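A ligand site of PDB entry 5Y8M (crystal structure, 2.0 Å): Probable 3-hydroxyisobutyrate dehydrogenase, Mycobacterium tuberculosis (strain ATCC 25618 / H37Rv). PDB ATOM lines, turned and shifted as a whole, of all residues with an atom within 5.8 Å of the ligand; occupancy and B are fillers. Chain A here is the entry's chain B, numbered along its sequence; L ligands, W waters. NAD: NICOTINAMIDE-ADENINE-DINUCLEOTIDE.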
ATOM      1  N   LEU A   8     -19.966 -23.334 -36.260  1.00  0.00           N
ATOM      2  CA  LEU A   8     -19.001 -22.499 -35.558  1.00  0.00           C
ATOM      3  C   LEU A   8     -18.722 -23.111 -34.187  1.00  0.00           C
ATOM      4  O   LEU A   8     -19.614 -23.127 -33.299  1.00  0.00           O
ATOM      5  CB  LEU A   8     -19.542 -21.083 -35.397  1.00  0.00           C
ATOM      6  CG  LEU A   8     -20.116 -20.478 -36.648  1.00  0.00           C
ATOM      7  CD1 LEU A   8     -20.643 -19.077 -36.391  1.00  0.00           C
ATOM      8  CD2 LEU A   8     -19.054 -20.398 -37.733  1.00  0.00           C
ATOM      9  N   GLY A   9     -17.526 -23.641 -34.008  1.00  0.00           N
ATOM     10  CA  GLY A   9     -17.195 -24.410 -32.787  1.00  0.00           C
ATOM     11  C   GLY A   9     -17.091 -25.855 -33.134  1.00  0.00           C
ATOM     12  O   GLY A   9     -18.119 -26.552 -33.159  1.00  0.00           O
ATOM     13  N   LEU A  10     -15.843 -26.323 -33.391  1.00  0.00           N
ATOM     14  CA  LEU A  10     -15.559 -27.642 -33.898  1.00  0.00           C
ATOM     15  C   LEU A  10     -14.684 -28.413 -32.904  1.00  0.00           C
ATOM     16  O   LEU A  10     -13.760 -29.089 -33.272  1.00  0.00           O
ATOM     17  CB  LEU A  10     -14.868 -27.562 -35.265  1.00  0.00           C
ATOM     18  CG  LEU A  10     -15.679 -26.891 -36.364  1.00  0.00           C
ATOM     19  CD1 LEU A  10     -14.801 -26.559 -37.557  1.00  0.00           C
ATOM     20  CD2 LEU A  10     -16.880 -27.730 -36.776  1.00  0.00           C
ATOM     21  N   GLY A  11     -14.999 -28.245 -31.633  1.00  0.00           N
ATOM     22  CA  GLY A  11     -14.262 -28.859 -30.526  1.00  0.00           C
ATOM     23  C   GLY A  11     -14.706 -30.247 -30.173  1.00  0.00           C
ATOM     24  O   GLY A  11     -15.123 -30.968 -31.003  1.00  0.00           O
ATOM     25  N   ASN A  12     -14.534 -30.638 -28.936  1.00  0.00           N
ATOM     26  CA  ASN A  12     -14.905 -31.981 -28.487  1.00  0.00           C
ATOM     27  C   ASN A  12     -16.333 -32.411 -28.870  1.00  0.00           C
ATOM     28  O   ASN A  12     -16.552 -33.513 -29.169  1.00  0.00           O
ATOM     29  CB  ASN A  12     -14.642 -32.159 -27.003  1.00  0.00           C
ATOM     30  CG  ASN A  12     -13.156 -32.096 -26.676  1.00  0.00           C
ATOM     31  OD1 ASN A  12     -12.369 -32.573 -27.404  1.00  0.00           O
ATOM     32  ND2 ASN A  12     -12.826 -31.483 -25.638  1.00  0.00           N
ATOM     33  N   MET A  13     -17.243 -31.478 -28.876  1.00  0.00           N
ATOM     34  CA  MET A  13     -18.612 -31.722 -29.179  1.00  0.00           C
ATOM     35  C   MET A  13     -18.894 -31.366 -30.641  1.00  0.00           C
ATOM     36  O   MET A  13     -19.443 -32.184 -31.378  1.00  0.00           O
ATOM     37  CB  MET A  13     -19.525 -30.960 -28.236  1.00  0.00           C
ATOM     38  CG  MET A  13     -19.525 -31.441 -26.781  1.00  0.00           C
ATOM     39  SD  MET A  13     -20.177 -33.137 -26.633  1.00  0.00           S
ATOM     40  CE  MET A  13     -21.927 -32.865 -26.762  1.00  0.00           C
ATOM     41  N   GLY A  14     -18.493 -30.181 -31.065  1.00  0.00           N
ATOM     42  CA  GLY A  14     -18.713 -29.786 -32.445  1.00  0.00           C
ATOM     43  C   GLY A  14     -18.131 -30.662 -33.547  1.00  0.00           C
ATOM     44  O   GLY A  14     -18.749 -30.847 -34.601  1.00  0.00           O
ATOM     45  N   PHE A  31     -16.066 -23.100 -39.034  1.00  0.00           N
ATOM     46  CA  PHE A  31     -15.030 -22.246 -38.594  1.00  0.00           C
ATOM     47  C   PHE A  31     -14.740 -22.546 -37.122  1.00  0.00           C
ATOM     48  O   PHE A  31     -15.669 -22.752 -36.322  1.00  0.00           O
ATOM     49  CB  PHE A  31     -15.393 -20.779 -38.786  1.00  0.00           C
ATOM     50  CG  PHE A  31     -14.402 -19.861 -38.147  1.00  0.00           C
ATOM     51  CD1 PHE A  31     -13.180 -19.591 -38.775  1.00  0.00           C
ATOM     52  CD2 PHE A  31     -14.627 -19.373 -36.876  1.00  0.00           C
ATOM     53  CE1 PHE A  31     -12.221 -18.819 -38.161  1.00  0.00           C
ATOM     54  CE2 PHE A  31     -13.707 -18.535 -36.295  1.00  0.00           C
ATOM     55  CZ  PHE A  31     -12.484 -18.274 -36.928  1.00  0.00           C
ATOM     56  N   ASP A  32     -13.467 -22.521 -36.753  1.00  0.00           N
ATOM     57  CA  ASP A  32     -13.070 -22.565 -35.363  1.00  0.00           C
ATOM     58  C   ASP A  32     -11.695 -21.944 -35.342  1.00  0.00           C
ATOM     59  O   ASP A  32     -10.849 -22.321 -36.166  1.00  0.00           O
ATOM     60  CB  ASP A  32     -13.004 -24.037 -34.964  1.00  0.00           C
ATOM     61  CG  ASP A  32     -12.675 -24.271 -33.472  1.00  0.00           C
ATOM     62  OD1 ASP A  32     -13.392 -25.051 -32.803  1.00  0.00           O
ATOM     63  OD2 ASP A  32     -11.712 -23.665 -32.990  1.00  0.00           O
ATOM     64  N   PRO A  33     -11.433 -21.009 -34.432  1.00  0.00           N
ATOM     65  CA  PRO A  33     -10.093 -20.348 -34.461  1.00  0.00           C
ATOM     66  C   PRO A  33      -8.950 -21.221 -33.881  1.00  0.00           C
ATOM     67  O   PRO A  33      -7.813 -20.823 -33.966  1.00  0.00           O
ATOM     68  CB  PRO A  33     -10.306 -19.134 -33.517  1.00  0.00           C
ATOM     69  CG  PRO A  33     -11.365 -19.639 -32.560  1.00  0.00           C
ATOM     70  CD  PRO A  33     -12.304 -20.396 -33.424  1.00  0.00           C
ATOM     71  N   ALA A  34      -9.231 -22.360 -33.300  1.00  0.00           N
ATOM     72  CA  ALA A  34      -8.194 -23.273 -32.937  1.00  0.00           C
ATOM     73  C   ALA A  34      -7.918 -24.185 -34.166  1.00  0.00           C
ATOM     74  O   ALA A  34      -8.761 -24.961 -34.569  1.00  0.00           O
ATOM     75  CB  ALA A  34      -8.589 -24.083 -31.738  1.00  0.00           C
ATOM     76  N   ALA A  37      -8.647 -28.046 -34.051  1.00  0.00           N
ATOM     77  CA  ALA A  37     -10.035 -28.392 -34.172  1.00  0.00           C
ATOM     78  C   ALA A  37     -10.473 -28.292 -35.636  1.00  0.00           C
ATOM     79  O   ALA A  37     -11.035 -29.229 -36.167  1.00  0.00           O
ATOM     80  CB  ALA A  37     -10.886 -27.479 -33.293  1.00  0.00           C
ATOM     81  N   ALA A  52     -15.321 -16.633 -39.401  1.00  0.00           N
ATOM     82  CA  ALA A  52     -16.703 -16.986 -39.101  1.00  0.00           C
ATOM     83  C   ALA A  52     -17.657 -16.298 -40.044  1.00  0.00           C
ATOM     84  O   ALA A  52     -18.534 -16.978 -40.559  1.00  0.00           O
ATOM     85  CB  ALA A  52     -17.031 -16.680 -37.641  1.00  0.00           C
ATOM     86  N   MET A  65     -21.483 -24.140 -31.182  1.00  0.00           N
ATOM     87  CA  MET A  65     -21.186 -25.120 -30.161  1.00  0.00           C
ATOM     88  C   MET A  65     -19.934 -24.623 -29.434  1.00  0.00           C
ATOM     89  O   MET A  65     -18.802 -25.044 -29.716  1.00  0.00           O
ATOM     90  CB  MET A  65     -21.019 -26.519 -30.775  1.00  0.00           C
ATOM     91  CG  MET A  65     -21.027 -27.593 -29.723  1.00  0.00           C
ATOM     92  SD  MET A  65     -22.509 -27.438 -28.671  1.00  0.00           S
ATOM     93  CE  MET A  65     -22.610 -29.068 -27.953  1.00  0.00           C
ATOM     94  N   LEU A  66     -20.162 -23.631 -28.544  1.00  0.00           N
ATOM     95  CA  LEU A  66     -19.132 -22.776 -28.052  1.00  0.00           C
ATOM     96  C   LEU A  66     -19.068 -22.832 -26.524  1.00  0.00           C
ATOM     97  O   LEU A  66     -20.017 -23.213 -25.904  1.00  0.00           O
ATOM     98  CB  LEU A  66     -19.393 -21.380 -28.511  1.00  0.00           C
ATOM     99  CG  LEU A  66     -19.323 -21.124 -29.995  1.00  0.00           C
ATOM    100  CD1 LEU A  66     -19.964 -19.790 -30.274  1.00  0.00           C
ATOM    101  CD2 LEU A  66     -17.863 -21.188 -30.472  1.00  0.00           C
ATOM    102  N   PRO A  67     -17.930 -22.435 -25.929  1.00  0.00           N
ATOM    103  CA  PRO A  67     -17.695 -22.656 -24.514  1.00  0.00           C
ATOM    104  C   PRO A  67     -18.543 -21.883 -23.520  1.00  0.00           C
ATOM    105  O   PRO A  67     -18.840 -22.443 -22.502  1.00  0.00           O
ATOM    106  CB  PRO A  67     -16.202 -22.294 -24.337  1.00  0.00           C
ATOM    107  CG  PRO A  67     -15.641 -22.099 -25.707  1.00  0.00           C
ATOM    108  CD  PRO A  67     -16.783 -21.766 -26.585  1.00  0.00           C
ATOM    109  N   THR A  68     -18.870 -20.598 -23.778  1.00  0.00           N
ATOM    110  CA  THR A  68     -19.529 -19.726 -22.829  1.00  0.00           C
ATOM    111  C   THR A  68     -20.484 -18.769 -23.488  1.00  0.00           C
ATOM    112  O   THR A  68     -20.426 -18.504 -24.683  1.00  0.00           O
ATOM    113  CB  THR A  68     -18.530 -18.833 -22.062  1.00  0.00           C
ATOM    114  OG1 THR A  68     -17.887 -17.920 -22.943  1.00  0.00           O
ATOM    115  CG2 THR A  68     -17.490 -19.649 -21.358  1.00  0.00           C
ATOM    116  N   VAL A  71     -18.674 -15.965 -25.254  1.00  0.00           N
ATOM    117  CA  VAL A  71     -18.138 -16.357 -26.593  1.00  0.00           C
ATOM    118  C   VAL A  71     -19.313 -16.395 -27.616  1.00  0.00           C
ATOM    119  O   VAL A  71     -19.165 -16.011 -28.769  1.00  0.00           O
ATOM    120  CB  VAL A  71     -17.385 -17.698 -26.529  1.00  0.00           C
ATOM    121  CG1 VAL A  71     -16.925 -18.142 -27.917  1.00  0.00           C
ATOM    122  CG2 VAL A  71     -16.152 -17.609 -25.621  1.00  0.00           C
ATOM    123  N   CYS A  75     -19.523 -14.053 -30.824  1.00  0.00           N
ATOM    124  CA  CYS A  75     -19.658 -14.687 -32.109  1.00  0.00           C
ATOM    125  C   CYS A  75     -20.883 -14.124 -32.879  1.00  0.00           C
ATOM    126  O   CYS A  75     -20.780 -13.744 -34.072  1.00  0.00           O
ATOM    127  CB  CYS A  75     -19.775 -16.214 -31.904  1.00  0.00           C
ATOM    128  SG  CYS A  75     -20.256 -17.137 -33.383  1.00  0.00           S
ATOM    129  N   SER A  92     -26.318 -24.599 -29.710  1.00  0.00           N
ATOM    130  CA  SER A  92     -26.283 -25.831 -28.881  1.00  0.00           C
ATOM    131  C   SER A  92     -25.258 -25.769 -27.767  1.00  0.00           C
ATOM    132  O   SER A  92     -25.133 -26.724 -27.039  1.00  0.00           O
ATOM    133  CB  SER A  92     -26.130 -27.072 -29.766  1.00  0.00           C
ATOM    134  OG  SER A  92     -27.309 -27.284 -30.535  1.00  0.00           O
ATOM    135  N   SER A  93     -24.576 -24.622 -27.571  1.00  0.00           N
ATOM    136  CA  SER A  93     -23.787 -24.351 -26.371  1.00  0.00           C
ATOM    137  C   SER A  93     -24.676 -24.424 -25.095  1.00  0.00           C
ATOM    138  O   SER A  93     -25.910 -24.241 -25.134  1.00  0.00           O
ATOM    139  CB  SER A  93     -23.141 -22.956 -26.456  1.00  0.00           C
ATOM    140  OG  SER A  93     -22.702 -22.599 -27.750  1.00  0.00           O
ATOM    141  N   THR A  94     -24.038 -24.697 -23.975  1.00  0.00           N
ATOM    142  CA  THR A  94     -24.657 -24.600 -22.707  1.00  0.00           C
ATOM    143  C   THR A  94     -24.304 -23.259 -22.083  1.00  0.00           C
ATOM    144  O   THR A  94     -23.122 -23.002 -21.772  1.00  0.00           O
ATOM    145  CB  THR A  94     -24.181 -25.734 -21.795  1.00  0.00           C
ATOM    146  OG1 THR A  94     -24.520 -26.959 -22.422  1.00  0.00           O
ATOM    147  CG2 THR A  94     -24.919 -25.679 -20.475  1.00  0.00           C
ATOM    148  N   ILE A  95     -25.306 -22.383 -21.919  1.00  0.00           N
ATOM    149  CA  ILE A  95     -25.053 -21.007 -21.477  1.00  0.00           C
ATOM    150  C   ILE A  95     -26.171 -20.601 -20.527  1.00  0.00           C
ATOM    151  O   ILE A  95     -27.196 -21.275 -20.478  1.00  0.00           O
ATOM    152  CB  ILE A  95     -24.858 -19.991 -22.650  1.00  0.00           C
ATOM    153  CG1 ILE A  95     -26.164 -19.652 -23.397  1.00  0.00           C
ATOM    154  CG2 ILE A  95     -23.784 -20.444 -23.631  1.00  0.00           C
ATOM    155  CD1 ILE A  95     -25.996 -18.609 -24.473  1.00  0.00           C
ATOM    156  N   VAL A 119     -27.476 -29.634 -25.277  1.00  0.00           N
ATOM    157  CA  VAL A 119     -27.519 -31.072 -25.436  1.00  0.00           C
ATOM    158  C   VAL A 119     -27.029 -31.759 -24.191  1.00  0.00           C
ATOM    159  O   VAL A 119     -26.241 -31.177 -23.375  1.00  0.00           O
ATOM    160  CB  VAL A 119     -26.702 -31.588 -26.635  1.00  0.00           C
ATOM    161  CG1 VAL A 119     -27.213 -30.925 -27.938  1.00  0.00           C
ATOM    162  CG2 VAL A 119     -25.212 -31.315 -26.490  1.00  0.00           C
ATOM    163  N   SER A 120     -27.436 -32.999 -24.044  1.00  0.00           N
ATOM    164  CA  SER A 120     -26.781 -33.921 -23.115  1.00  0.00           C
ATOM    165  C   SER A 120     -26.321 -35.174 -23.856  1.00  0.00           C
ATOM    166  O   SER A 120     -26.919 -35.554 -24.870  1.00  0.00           O
ATOM    167  CB  SER A 120     -27.763 -34.254 -22.018  1.00  0.00           C
ATOM    168  OG  SER A 120     -28.756 -35.060 -22.536  1.00  0.00           O
ATOM    169  N   GLY A 121     -25.267 -35.823 -23.340  1.00  0.00           N
ATOM    170  CA  GLY A 121     -24.772 -37.055 -23.906  1.00  0.00           C
ATOM    171  C   GLY A 121     -23.282 -37.121 -24.016  1.00  0.00           C
ATOM    172  O   GLY A 121     -22.733 -38.190 -24.199  1.00  0.00           O
ATOM    173  N   GLY A 122     -22.636 -35.981 -23.887  1.00  0.00           N
ATOM    174  CA  GLY A 122     -21.198 -35.882 -24.036  1.00  0.00           C
ATOM    175  C   GLY A 122     -20.707 -36.279 -25.414  1.00  0.00           C
ATOM    176  O   GLY A 122     -21.463 -36.408 -26.385  1.00  0.00           O
ATOM    177  N   VAL A 123     -19.411 -36.456 -25.460  1.00  0.00           N
ATOM    178  CA  VAL A 123     -18.717 -36.750 -26.655  1.00  0.00           C
ATOM    179  C   VAL A 123     -19.135 -38.109 -27.249  1.00  0.00           C
ATOM    180  O   VAL A 123     -19.165 -38.238 -28.480  1.00  0.00           O
ATOM    181  CB  VAL A 123     -17.203 -36.680 -26.439  1.00  0.00           C
ATOM    182  CG1 VAL A 123     -16.488 -37.168 -27.667  1.00  0.00           C
ATOM    183  CG2 VAL A 123     -16.753 -35.231 -26.220  1.00  0.00           C
ATOM    184  N   LYS A 169     -32.295 -27.999 -19.108  1.00  0.00           N
ATOM    185  CA  LYS A 169     -30.996 -28.588 -18.872  1.00  0.00           C
ATOM    186  C   LYS A 169     -30.445 -28.274 -17.486  1.00  0.00           C
ATOM    187  O   LYS A 169     -29.973 -29.174 -16.775  1.00  0.00           O
ATOM    188  CB  LYS A 169     -29.940 -28.140 -19.889  1.00  0.00           C
ATOM    189  CG  LYS A 169     -28.776 -29.097 -19.879  1.00  0.00           C
ATOM    190  CD  LYS A 169     -27.688 -28.789 -20.897  1.00  0.00           C
ATOM    191  CE  LYS A 169     -26.340 -29.221 -20.343  1.00  0.00           C
ATOM    192  NZ  LYS A 169     -25.372 -29.602 -21.383  1.00  0.00           N
ATOM    193  N   GLY A 236     -16.812 -40.331 -18.719  1.00  0.00           N
ATOM    194  CA  GLY A 236     -17.981 -39.875 -17.943  1.00  0.00           C
ATOM    195  C   GLY A 236     -18.297 -38.389 -18.135  1.00  0.00           C
ATOM    196  O   GLY A 236     -18.217 -37.873 -19.247  1.00  0.00           O
ATOM    197  N   LEU A 241     -17.069 -30.029 -16.047  1.00  0.00           N
ATOM    198  CA  LEU A 241     -18.312 -29.705 -16.723  1.00  0.00           C
ATOM    199  C   LEU A 241     -19.489 -29.558 -15.730  1.00  0.00           C
ATOM    200  O   LEU A 241     -20.330 -28.627 -15.876  1.00  0.00           O
ATOM    201  CB  LEU A 241     -18.648 -30.749 -17.794  1.00  0.00           C
ATOM    202  CG  LEU A 241     -17.903 -30.564 -19.107  1.00  0.00           C
ATOM    203  CD1 LEU A 241     -18.066 -31.794 -20.026  1.00  0.00           C
ATOM    204  CD2 LEU A 241     -18.418 -29.279 -19.766  1.00  0.00           C
ATOM    205  N   LYS A 244     -19.226 -26.246 -14.168  1.00  0.00           N
ATOM    206  CA  LYS A 244     -19.770 -25.219 -15.083  1.00  0.00           C
ATOM    207  C   LYS A 244     -21.302 -25.142 -15.053  1.00  0.00           C
ATOM    208  O   LYS A 244     -21.895 -24.050 -14.929  1.00  0.00           O
ATOM    209  CB  LYS A 244     -19.301 -25.495 -16.500  1.00  0.00           C
ATOM    210  CG  LYS A 244     -19.817 -24.506 -17.532  1.00  0.00           C
ATOM    211  CD  LYS A 244     -19.933 -25.142 -18.933  1.00  0.00           C
ATOM    212  CE  LYS A 244     -20.075 -24.035 -19.960  1.00  0.00           C
ATOM    213  NZ  LYS A 244     -20.837 -24.374 -21.162  1.00  0.00           N
ATOM    214  N   ASP A 245     -21.943 -26.300 -15.170  1.00  0.00           N
ATOM    215  CA  ASP A 245     -23.425 -26.334 -15.200  1.00  0.00           C
ATOM    216  C   ASP A 245     -24.025 -25.859 -13.889  1.00  0.00           C
ATOM    217  O   ASP A 245     -25.071 -25.217 -13.876  1.00  0.00           O
ATOM    218  CB  ASP A 245     -23.936 -27.731 -15.492  1.00  0.00           C
ATOM    219  CG  ASP A 245     -23.719 -28.182 -16.944  1.00  0.00           C
ATOM    220  OD1 ASP A 245     -23.361 -27.370 -17.815  1.00  0.00           O
ATOM    221  OD2 ASP A 245     -23.880 -29.378 -17.197  1.00  0.00           O
HETATM  222  PA  NAD L   1     -14.406 -27.259 -26.664  1.00  0.00           P
HETATM  223  O1A NAD L   1     -13.708 -26.170 -25.877  1.00  0.00           O
HETATM  224  O2A NAD L   1     -13.869 -28.666 -26.928  1.00  0.00           O
HETATM  225  O5B NAD L   1     -14.871 -26.616 -28.053  1.00  0.00           O
HETATM  226  C5B NAD L   1     -15.226 -25.250 -28.203  1.00  0.00           C
HETATM  227  C4B NAD L   1     -14.648 -24.799 -29.533  1.00  0.00           C
HETATM  228  O4B NAD L   1     -15.162 -23.516 -29.902  1.00  0.00           O
HETATM  229  C3B NAD L   1     -13.110 -24.721 -29.465  1.00  0.00           C
HETATM  230  O3B NAD L   1     -12.510 -25.620 -30.441  1.00  0.00           O
HETATM  231  C2B NAD L   1     -12.875 -23.218 -29.679  1.00  0.00           C
HETATM  232  O2B NAD L   1     -11.704 -22.817 -30.404  1.00  0.00           O
HETATM  233  C1B NAD L   1     -14.084 -22.839 -30.499  1.00  0.00           C
HETATM  234  N9A NAD L   1     -14.362 -21.405 -30.552  1.00  0.00           N
HETATM  235  C8A NAD L   1     -14.148 -20.468 -29.603  1.00  0.00           C
HETATM  236  N7A NAD L   1     -14.573 -19.255 -30.065  1.00  0.00           N
HETATM  237  C5A NAD L   1     -15.075 -19.434 -31.279  1.00  0.00           C
HETATM  238  C6A NAD L   1     -15.730 -18.650 -32.309  1.00  0.00           C
HETATM  239  N6A NAD L   1     -15.955 -17.349 -32.157  1.00  0.00           N
HETATM  240  N1A NAD L   1     -16.141 -19.219 -33.432  1.00  0.00           N
HETATM  241  C2A NAD L   1     -15.967 -20.509 -33.649  1.00  0.00           C
HETATM  242  N3A NAD L   1     -15.409 -21.302 -32.770  1.00  0.00           N
HETATM  243  C4A NAD L   1     -14.944 -20.850 -31.590  1.00  0.00           C
HETATM  244  O3  NAD L   1     -15.836 -27.392 -25.944  1.00  0.00           O
HETATM  245  PN  NAD L   1     -16.888 -28.580 -26.205  1.00  0.00           P
HETATM  246  O1N NAD L   1     -16.570 -29.733 -25.265  1.00  0.00           O
HETATM  247  O2N NAD L   1     -17.077 -28.862 -27.712  1.00  0.00           O
HETATM  248  O5D NAD L   1     -18.228 -27.954 -25.592  1.00  0.00           O
HETATM  249  C5D NAD L   1     -18.957 -26.926 -26.301  1.00  0.00           C
HETATM  250  C4D NAD L   1     -20.264 -26.679 -25.538  1.00  0.00           C
HETATM  251  O4D NAD L   1     -20.959 -27.901 -25.342  1.00  0.00           O
HETATM  252  C3D NAD L   1     -20.010 -26.069 -24.154  1.00  0.00           C
HETATM  253  O3D NAD L   1     -20.968 -24.956 -23.934  1.00  0.00           O
HETATM  254  C2D NAD L   1     -20.237 -27.228 -23.210  1.00  0.00           C
HETATM  255  O2D NAD L   1     -20.658 -26.811 -21.898  1.00  0.00           O
HETATM  256  C1D NAD L   1     -21.311 -28.053 -23.951  1.00  0.00           C
HETATM  257  N1N NAD L   1     -21.445 -29.489 -23.598  1.00  0.00           N
HETATM  258  C2N NAD L   1     -20.298 -30.251 -23.519  1.00  0.00           C
HETATM  259  C3N NAD L   1     -20.310 -31.647 -23.197  1.00  0.00           C
HETATM  260  C7N NAD L   1     -19.036 -32.445 -23.162  1.00  0.00           C
HETATM  261  O7N NAD L   1     -18.969 -33.587 -22.709  1.00  0.00           O
HETATM  262  N7N NAD L   1     -17.961 -31.933 -23.766  1.00  0.00           N
HETATM  263  C4N NAD L   1     -21.553 -32.259 -22.930  1.00  0.00           C
HETATM  264  C5N NAD L   1     -22.719 -31.484 -23.068  1.00  0.00           C
HETATM  265  C6N NAD L   1     -22.667 -30.099 -23.420  1.00  0.00           C
HETATM  266  O   HOH W   1     -25.018 -27.907 -24.691  1.00  0.00           O
HETATM  267  O   HOH W   2     -16.677 -15.481 -30.017  1.00  0.00           O
HETATM  268  O   HOH W   3     -12.211 -23.783 -25.981  1.00  0.00           O
HETATM  269  O   HOH W   4     -17.896 -35.843 -23.000  1.00  0.00           O
HETATM  270  O   HOH W   5     -16.281 -13.884 -32.279  1.00  0.00           O
HETATM  271  O   HOH W   6     -17.491 -16.743 -34.474  1.00  0.00           O
HETATM  272  O   HOH W   7     -17.396 -27.434 -29.984  1.00  0.00           O
HETATM  273  O   HOH W   8     -20.214 -34.873 -20.564  1.00  0.00           O
HETATM  274  O   HOH W   9     -12.401 -20.979 -26.660  1.00  0.00           O
HETATM  275  O   HOH W  10     -15.213 -33.244 -23.333  1.00  0.00           O
HETATM  276  O   HOH W  11      -9.770 -21.465 -29.266  1.00  0.00           O
HETATM  277  O   HOH W  12     -11.477 -28.660 -27.807  1.00  0.00           O
HETATM  278  O   HOH W  13     -10.401 -26.801 -29.419  1.00  0.00           O
HETATM  279  O   HOH W  14     -14.529 -30.611 -23.934  1.00  0.00           O
HETATM  280  O   HOH W  15     -22.187 -28.124 -20.244  1.00  0.00           O
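NZ of Lys 244 lies within hydrogen-bond range of O2D of the ligand (2.6 Å).
The side-chain carboxylate (OD1) of Asp 32 is in hydrogen-bond range of an oxygen (O3B) of the ligand (2.6 Å).
An oxygen (O3D) of the ligand sits at hydrogen-bond distance from the backbone carbonyl oxygen (O) of Leu 66 (2.8 Å).
O2N of the ligand sits at hydrogen-bond distance from N of Met 13 (2.9 Å).
The backbone NH (N) of Asn 12 lies within hydrogen-bond range of an oxygen (O2A) of the ligand (2.9 Å).
ND2 of Asn 12 is in hydrogen-bond range of O2A of the ligand.
An oxygen (O3D) of the ligand lies within hydrogen-bond range of the backbone NH of Thr 94 (3.1 Å).
The backbone NH (N) of Gly 9 is in hydrogen-bond range of a nitrogen (N3A) of the ligand, at 3.4 Å.
The side-chain amino group of Lys 244 is in hydrogen-bond range of the backbone carbonyl oxygen of Thr 94 (2.7 Å).
The side-chain amino group of Lys 244 is in hydrogen-bond range of the backbone carbonyl oxygen of Pro 67 (3.1 Å).
OD2 of Asp 32 lies within hydrogen-bond range of N of Ala 34 (2.8 Å).
OG of Ser 93 sits at hydrogen-bond distance from N of Leu 66 (2.9 Å).
The side-chain sulfur (SD) of Met 13 sits at hydrogen-bond distance from the backbone NH (N) of Val 123, 3.6 Å away.
The side-chain amino group (NZ) of Lys 169 is in hydrogen-bond range of the side-chain hydroxyl (OG1) of Thr 94.
N of Met 65 lies within hydrogen-bond range of O of Leu 8 (3.0 Å).
The side-chain amino group (NZ) of Lys 169 lies within hydrogen-bond range of the backbone carbonyl oxygen (O) of Val 119 (2.7 Å).
The side-chain sulfur of Met 65 lies close to an oxygen (O4D) of the ligand (3.7 Å).
Leu 8 touches the ligand.
CA of Gly 11 touches O5B of the ligand (3.4 Å).
N of Gly 14 touches O2N of the ligand, at 3.9 Å.
Phe 31 touches the ligand.
Pro 33 touches the ligand.
CB of Ala 34 touches O2B of the ligand, at 3.6 Å.
Ala 37 touches the ligand (CB to O3B, 3.8 Å).
O of Pro 67 touches O3D of the ligand, 3.6 Å away.
Val 71 touches the ligand (CG1 to N7A, 3.4 Å).
CB of Cys 75 touches N6A of the ligand, at 3.99 Å.
CA of Ser 93 touches O3D of the ligand, 3.8 Å away.
Val 119 touches the ligand.
CA of Gly 122 touches O7N of the ligand, 3.5 Å away.
Val 123 touches the ligand (N to O7N, 3.999 Å).
Lys 169 touches the ligand.
Leu 241 touches the ligand.
Hydrophobic or aromatic side chains that line the ligand: Met 13, Phe 31, Pro 33, Ala 34, Ala 37, Met 65, Leu 66, Val 71 and Leu 241.
Within 4 Å of the ligand: Leu 8, Gly 9, Gly 11, Asn 12, Met 13, Gly 14, Phe 31, Asp 32, Pro 33, Ala 34, Ala 37, Met 65, Leu 66, Pro 67, Val 71, Cys 75, Ser 93, Thr 94, Val 119, Gly 122, Val 123, Lys 169, Leu 241 and Lys 244.
Water W4 bridges O7N of the ligand (2.5 Å) and N of Val 123 (3.0 Å).
Water W14 bridges the side-chain amide nitrogen of Asn 12 (2.6 Å) and an oxygen (O1N) of the ligand (2.6 Å).
Water W7 lies within hydrogen-bond range of an oxygen (O2N) of the ligand (2.7 Å), the backbone carbonyl oxygen (O) of Met 65 (2.8 Å), the backbone NH (N) of Gly 11 (3.0 Å), the backbone NH (N) of Gly 14 (3.1 Å) and the backbone carbonyl oxygen (O) of Gly 9 (3.4 Å).
Water W6 lies within hydrogen-bond range of N6A of the ligand and SG of Cys 75.
Water W2 lies within hydrogen-bond range of O of Val 71, N6A of the ligand and N of Cys 75.
Water W1 lies within hydrogen-bond range of the side-chain hydroxyl of Thr 94 (2.5 Å), the backbone carbonyl oxygen of Ser 92 (2.6 Å) and the backbone NH of Val 119 (3.1 Å).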
